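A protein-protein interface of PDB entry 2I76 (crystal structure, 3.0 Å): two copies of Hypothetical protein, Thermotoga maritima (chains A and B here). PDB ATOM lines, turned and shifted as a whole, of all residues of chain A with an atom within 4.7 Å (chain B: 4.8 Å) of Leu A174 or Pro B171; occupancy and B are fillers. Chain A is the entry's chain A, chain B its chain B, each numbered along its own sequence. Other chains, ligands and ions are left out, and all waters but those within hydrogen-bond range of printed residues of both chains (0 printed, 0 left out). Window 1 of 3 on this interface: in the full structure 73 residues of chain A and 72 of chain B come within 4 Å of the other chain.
Among the printed residues, 9 pairs touch across the chains.
OG of Ser A178 sits close to O of Ile B166 (3.1 Å).
The backbone carbonyl oxygen (O) of Ile B166 lies close to the backbone carbonyl oxygen (O) of Leu A174 (3.4 Å).
Pro A171 touches Leu B174, and with the chains exchanged Leu A174 touches Pro B171.
Leu A174 touches Phe B170, but with the chains exchanged Phe A170 does not touch Leu B174 (4.04 Å).
Leu A174 touches its own counterpart, Leu B174.
7 positions are printed for both chains.
Printed residues of chain B within 4 Å of Pro A171: Leu B174.
Ala A173 touches none of the printed residues of chain B.
Of chain B, only Ile B166, Phe B170, Pro B171 and Leu B174 come within 4 Å of Leu A174.
Of the printed residues of chain B, Leu A177 touches Ile B166.
Of the printed residues of chain B, Ser A178 touches Ile B166 and Ala B167.
Printed residues of chain B within 4 Å of Met A198: Ala B167.
Of chain A, only Leu A174 comes within 4 Å of Pro B171.
The nearest printed residue of chain B that does not touch Pro A171 is Met B198 (4.7 Å).
The backbone carbonyl oxygen (O) of Leu A174 sits at hydrogen-bond distance from the side-chain hydroxyl (OG) of Ser A178 (3.3 Å).
The backbone carbonyl oxygen of Val B165 is in hydrogen-bond range of the backbone NH of Phe B170 (3.0 Å).
Among the printed residues, merely in contact across the chains: Leu A174 with Leu B174 (3.1 Å), Leu A174 with Pro B171 (3.3 Å), Met A198 with Ala B167 (3.5 Å), Ser A178 with Ala B167 (3.5 Å), Leu A177 with Ile B166 (3.6 Å), Leu A174 with Phe B170 (3.8 Å) and Pro A171 with Leu B174 (3.9 Å).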
ATOM      1  N   PHE A 170       9.161 -35.229  31.832  1.00  0.00           N
ATOM      2  CA  PHE A 170       8.896 -33.835  32.150  1.00  0.00           C
ATOM      3  C   PHE A 170       9.326 -32.763  31.154  1.00  0.00           C
ATOM      4  O   PHE A 170       8.567 -31.825  30.892  1.00  0.00           O
ATOM      5  CB  PHE A 170       9.424 -33.525  33.546  1.00  0.00           C
ATOM      6  CG  PHE A 170       8.540 -34.063  34.645  1.00  0.00           C
ATOM      7  CD1 PHE A 170       8.601 -33.539  35.939  1.00  0.00           C
ATOM      8  CD2 PHE A 170       7.594 -35.051  34.366  1.00  0.00           C
ATOM      9  CE1 PHE A 170       7.741 -33.992  36.934  1.00  0.00           C
ATOM     10  CE2 PHE A 170       6.733 -35.508  35.349  1.00  0.00           C
ATOM     11  CZ  PHE A 170       6.801 -34.971  36.638  1.00  0.00           C
ATOM     12  N   PRO A 171      10.531 -32.880  30.576  1.00  0.00           N
ATOM     13  CA  PRO A 171      10.931 -31.852  29.622  1.00  0.00           C
ATOM     14  C   PRO A 171       9.897 -31.676  28.522  1.00  0.00           C
ATOM     15  O   PRO A 171       9.635 -30.570  28.053  1.00  0.00           O
ATOM     16  CB  PRO A 171      12.250 -32.386  29.107  1.00  0.00           C
ATOM     17  CG  PRO A 171      12.834 -32.978  30.339  1.00  0.00           C
ATOM     18  CD  PRO A 171      11.659 -33.781  30.857  1.00  0.00           C
ATOM     19  N   VAL A 172       9.309 -32.786  28.108  1.00  0.00           N
ATOM     20  CA  VAL A 172       8.293 -32.765  27.075  1.00  0.00           C
ATOM     21  C   VAL A 172       7.210 -31.720  27.337  1.00  0.00           C
ATOM     22  O   VAL A 172       6.749 -31.064  26.401  1.00  0.00           O
ATOM     23  CB  VAL A 172       7.663 -34.148  26.941  1.00  0.00           C
ATOM     24  CG1 VAL A 172       6.498 -34.112  25.973  1.00  0.00           C
ATOM     25  CG2 VAL A 172       8.725 -35.109  26.462  1.00  0.00           C
ATOM     26  N   ALA A 173       6.802 -31.556  28.596  1.00  0.00           N
ATOM     27  CA  ALA A 173       5.774 -30.573  28.919  1.00  0.00           C
ATOM     28  C   ALA A 173       6.320 -29.197  28.619  1.00  0.00           C
ATOM     29  O   ALA A 173       5.567 -28.269  28.384  1.00  0.00           O
ATOM     30  CB  ALA A 173       5.377 -30.663  30.368  1.00  0.00           C
ATOM     31  N   LEU A 174       7.637 -29.057  28.629  1.00  0.00           N
ATOM     32  CA  LEU A 174       8.228 -27.764  28.329  1.00  0.00           C
ATOM     33  C   LEU A 174       8.253 -27.579  26.809  1.00  0.00           C
ATOM     34  O   LEU A 174       7.971 -26.493  26.294  1.00  0.00           O
ATOM     35  CB  LEU A 174       9.640 -27.664  28.928  1.00  0.00           C
ATOM     36  CG  LEU A 174       9.754 -27.799  30.456  1.00  0.00           C
ATOM     37  CD1 LEU A 174      11.200 -27.724  30.897  1.00  0.00           C
ATOM     38  CD2 LEU A 174       8.975 -26.692  31.122  1.00  0.00           C
ATOM     39  N   ALA A 175       8.579 -28.642  26.086  1.00  0.00           N
ATOM     40  CA  ALA A 175       8.613 -28.566  24.634  1.00  0.00           C
ATOM     41  C   ALA A 175       7.204 -28.250  24.125  1.00  0.00           C
ATOM     42  O   ALA A 175       7.021 -27.543  23.141  1.00  0.00           O
ATOM     43  CB  ALA A 175       9.104 -29.894  24.053  1.00  0.00           C
ATOM     44  N   TYR A 176       6.205 -28.769  24.826  1.00  0.00           N
ATOM     45  CA  TYR A 176       4.802 -28.587  24.449  1.00  0.00           C
ATOM     46  C   TYR A 176       4.362 -27.134  24.590  1.00  0.00           C
ATOM     47  O   TYR A 176       3.764 -26.549  23.679  1.00  0.00           O
ATOM     48  CB  TYR A 176       3.953 -29.500  25.329  1.00  0.00           C
ATOM     49  CG  TYR A 176       2.463 -29.277  25.256  1.00  0.00           C
ATOM     50  CD1 TYR A 176       1.680 -29.889  24.262  1.00  0.00           C
ATOM     51  CD2 TYR A 176       1.805 -28.523  26.247  1.00  0.00           C
ATOM     52  CE1 TYR A 176       0.281 -29.766  24.274  1.00  0.00           C
ATOM     53  CE2 TYR A 176       0.415 -28.394  26.260  1.00  0.00           C
ATOM     54  CZ  TYR A 176      -0.334 -29.022  25.279  1.00  0.00           C
ATOM     55  OH  TYR A 176      -1.700 -28.931  25.335  1.00  0.00           O
ATOM     56  N   LEU A 177       4.663 -26.558  25.748  1.00  0.00           N
ATOM     57  CA  LEU A 177       4.321 -25.172  26.022  1.00  0.00           C
ATOM     58  C   LEU A 177       4.906 -24.214  24.988  1.00  0.00           C
ATOM     59  O   LEU A 177       4.208 -23.319  24.518  1.00  0.00           O
ATOM     60  CB  LEU A 177       4.809 -24.772  27.411  1.00  0.00           C
ATOM     61  CG  LEU A 177       3.914 -25.250  28.547  1.00  0.00           C
ATOM     62  CD1 LEU A 177       4.587 -24.943  29.874  1.00  0.00           C
ATOM     63  CD2 LEU A 177       2.548 -24.566  28.453  1.00  0.00           C
ATOM     64  N   SER A 178       6.178 -24.401  24.641  1.00  0.00           N
ATOM     65  CA  SER A 178       6.831 -23.537  23.671  1.00  0.00           C
ATOM     66  C   SER A 178       6.311 -23.729  22.252  1.00  0.00           C
ATOM     67  O   SER A 178       6.053 -22.755  21.542  1.00  0.00           O
ATOM     68  CB  SER A 178       8.322 -23.782  23.682  1.00  0.00           C
ATOM     69  OG  SER A 178       8.836 -23.558  24.966  1.00  0.00           O
ATOM     70  N   MET A 198      16.846 -26.352  23.653  1.00  0.00           N
ATOM     71  CA  MET A 198      16.951 -27.365  24.705  1.00  0.00           C
ATOM     72  C   MET A 198      18.209 -28.239  24.750  1.00  0.00           C
ATOM     73  O   MET A 198      18.667 -28.615  25.823  1.00  0.00           O
ATOM     74  CB  MET A 198      15.714 -28.266  24.637  1.00  0.00           C
ATOM     75  CG  MET A 198      15.229 -28.784  25.973  1.00  0.00           C
ATOM     76  SD  MET A 198      13.810 -30.099  25.797  1.00  0.00           S
ATOM     77  CE  MET A 198      12.427 -28.995  25.031  1.00  0.00           C
ATOM     78  N   LEU A 242       2.459 -23.306  36.616  1.00  0.00           N
ATOM     79  CA  LEU A 242       3.740 -23.884  36.234  1.00  0.00           C
ATOM     80  C   LEU A 242       4.838 -22.841  36.146  1.00  0.00           C
ATOM     81  O   LEU A 242       5.966 -23.071  36.581  1.00  0.00           O
ATOM     82  CB  LEU A 242       3.642 -24.612  34.894  1.00  0.00           C
ATOM     83  CG  LEU A 242       4.959 -25.346  34.603  1.00  0.00           C
ATOM     84  CD1 LEU A 242       4.788 -26.819  34.870  1.00  0.00           C
ATOM     85  CD2 LEU A 242       5.394 -25.114  33.171  1.00  0.00           C
ATOM     86  N   VAL B 165      12.461 -18.977  26.924  1.00  0.00           N
ATOM     87  CA  VAL B 165      12.733 -19.242  28.328  1.00  0.00           C
ATOM     88  C   VAL B 165      12.165 -20.581  28.780  1.00  0.00           C
ATOM     89  O   VAL B 165      12.851 -21.340  29.465  1.00  0.00           O
ATOM     90  CB  VAL B 165      12.181 -18.135  29.229  1.00  0.00           C
ATOM     91  CG1 VAL B 165      12.043 -18.638  30.615  1.00  0.00           C
ATOM     92  CG2 VAL B 165      13.138 -16.955  29.234  1.00  0.00           C
ATOM     93  N   ILE B 166      10.923 -20.889  28.411  1.00  0.00           N
ATOM     94  CA  ILE B 166      10.365 -22.161  28.835  1.00  0.00           C
ATOM     95  C   ILE B 166      10.819 -23.265  27.913  1.00  0.00           C
ATOM     96  O   ILE B 166      10.112 -24.262  27.751  1.00  0.00           O
ATOM     97  CB  ILE B 166       8.810 -22.155  28.904  1.00  0.00           C
ATOM     98  CG1 ILE B 166       8.187 -22.009  27.537  1.00  0.00           C
ATOM     99  CG2 ILE B 166       8.338 -20.980  29.695  1.00  0.00           C
ATOM    100  CD1 ILE B 166       6.687 -21.676  27.617  1.00  0.00           C
ATOM    101  N   ALA B 167      12.005 -23.086  27.326  1.00  0.00           N
ATOM    102  CA  ALA B 167      12.589 -24.073  26.417  1.00  0.00           C
ATOM    103  C   ALA B 167      14.079 -24.276  26.641  1.00  0.00           C
ATOM    104  O   ALA B 167      14.609 -25.339  26.327  1.00  0.00           O
ATOM    105  CB  ALA B 167      12.351 -23.672  24.979  1.00  0.00           C
ATOM    106  N   SER B 168      14.751 -23.256  27.172  1.00  0.00           N
ATOM    107  CA  SER B 168      16.190 -23.326  27.431  1.00  0.00           C
ATOM    108  C   SER B 168      16.519 -22.877  28.859  1.00  0.00           C
ATOM    109  O   SER B 168      17.663 -22.972  29.315  1.00  0.00           O
ATOM    110  CB  SER B 168      16.941 -22.437  26.451  1.00  0.00           C
ATOM    111  OG  SER B 168      16.589 -21.088  26.677  1.00  0.00           O
ATOM    112  N   ASN B 169      15.525 -22.358  29.562  1.00  0.00           N
ATOM    113  CA  ASN B 169      15.755 -21.942  30.933  1.00  0.00           C
ATOM    114  C   ASN B 169      15.095 -22.951  31.853  1.00  0.00           C
ATOM    115  O   ASN B 169      15.757 -23.645  32.633  1.00  0.00           O
ATOM    116  CB  ASN B 169      15.171 -20.545  31.202  1.00  0.00           C
ATOM    117  CG  ASN B 169      16.092 -19.421  30.743  1.00  0.00           C
ATOM    118  OD1 ASN B 169      17.306 -19.497  30.910  1.00  0.00           O
ATOM    119  ND2 ASN B 169      15.512 -18.364  30.183  1.00  0.00           N
ATOM    120  N   PHE B 170      13.776 -23.042  31.734  1.00  0.00           N
ATOM    121  CA  PHE B 170      12.997 -23.939  32.571  1.00  0.00           C
ATOM    122  C   PHE B 170      13.575 -25.353  32.730  1.00  0.00           C
ATOM    123  O   PHE B 170      13.595 -25.884  33.844  1.00  0.00           O
ATOM    124  CB  PHE B 170      11.539 -23.974  32.078  1.00  0.00           C
ATOM    125  CG  PHE B 170      10.761 -22.709  32.391  1.00  0.00           C
ATOM    126  CD1 PHE B 170       9.371 -22.708  32.369  1.00  0.00           C
ATOM    127  CD2 PHE B 170      11.421 -21.530  32.760  1.00  0.00           C
ATOM    128  CE1 PHE B 170       8.657 -21.567  32.717  1.00  0.00           C
ATOM    129  CE2 PHE B 170      10.714 -20.381  33.109  1.00  0.00           C
ATOM    130  CZ  PHE B 170       9.335 -20.399  33.088  1.00  0.00           C
ATOM    131  N   PRO B 171      14.065 -25.974  31.635  1.00  0.00           N
ATOM    132  CA  PRO B 171      14.633 -27.319  31.704  1.00  0.00           C
ATOM    133  C   PRO B 171      15.667 -27.517  32.803  1.00  0.00           C
ATOM    134  O   PRO B 171      15.839 -28.626  33.322  1.00  0.00           O
ATOM    135  CB  PRO B 171      15.190 -27.514  30.304  1.00  0.00           C
ATOM    136  CG  PRO B 171      14.123 -26.920  29.493  1.00  0.00           C
ATOM    137  CD  PRO B 171      13.871 -25.592  30.227  1.00  0.00           C
ATOM    138  N   VAL B 172      16.360 -26.457  33.179  1.00  0.00           N
ATOM    139  CA  VAL B 172      17.327 -26.631  34.240  1.00  0.00           C
ATOM    140  C   VAL B 172      16.598 -26.918  35.555  1.00  0.00           C
ATOM    141  O   VAL B 172      17.093 -27.660  36.399  1.00  0.00           O
ATOM    142  CB  VAL B 172      18.224 -25.405  34.385  1.00  0.00           C
ATOM    143  CG1 VAL B 172      19.081 -25.549  35.625  1.00  0.00           C
ATOM    144  CG2 VAL B 172      19.124 -25.288  33.172  1.00  0.00           C
ATOM    145  N   ALA B 173      15.414 -26.338  35.724  1.00  0.00           N
ATOM    146  CA  ALA B 173      14.624 -26.572  36.934  1.00  0.00           C
ATOM    147  C   ALA B 173      14.247 -28.061  37.085  1.00  0.00           C
ATOM    148  O   ALA B 173      13.990 -28.546  38.190  1.00  0.00           O
ATOM    149  CB  ALA B 173      13.358 -25.708  36.919  1.00  0.00           C
ATOM    150  N   LEU B 174      14.193 -28.779  35.970  1.00  0.00           N
ATOM    151  CA  LEU B 174      13.885 -30.194  36.012  1.00  0.00           C
ATOM    152  C   LEU B 174      15.178 -30.937  36.276  1.00  0.00           C
ATOM    153  O   LEU B 174      15.264 -31.759  37.185  1.00  0.00           O
ATOM    154  CB  LEU B 174      13.288 -30.641  34.690  1.00  0.00           C
ATOM    155  CG  LEU B 174      11.792 -30.345  34.472  1.00  0.00           C
ATOM    156  CD1 LEU B 174      11.302 -29.239  35.398  1.00  0.00           C
ATOM    157  CD2 LEU B 174      11.577 -29.964  33.005  1.00  0.00           C
ATOM    158  N   ALA B 175      16.194 -30.636  35.480  1.00  0.00           N
ATOM    159  CA  ALA B 175      17.491 -31.277  35.660  1.00  0.00           C
ATOM    160  C   ALA B 175      17.898 -31.112  37.116  1.00  0.00           C
ATOM    161  O   ALA B 175      18.437 -32.031  37.734  1.00  0.00           O
ATOM    162  CB  ALA B 175      18.535 -30.642  34.740  1.00  0.00           C
ATOM    163  N   MET B 198      18.068 -36.249  29.431  1.00  0.00           N
ATOM    164  CA  MET B 198      17.625 -34.963  28.905  1.00  0.00           C
ATOM    165  C   MET B 198      18.057 -34.776  27.460  1.00  0.00           C
ATOM    166  O   MET B 198      17.314 -34.224  26.653  1.00  0.00           O
ATOM    167  CB  MET B 198      18.205 -33.842  29.751  1.00  0.00           C
ATOM    168  CG  MET B 198      17.529 -32.499  29.571  1.00  0.00           C
ATOM    169  SD  MET B 198      17.221 -31.692  31.308  1.00  0.00           S
ATOM    170  CE  MET B 198      17.493 -33.271  32.412  1.00  0.00           C
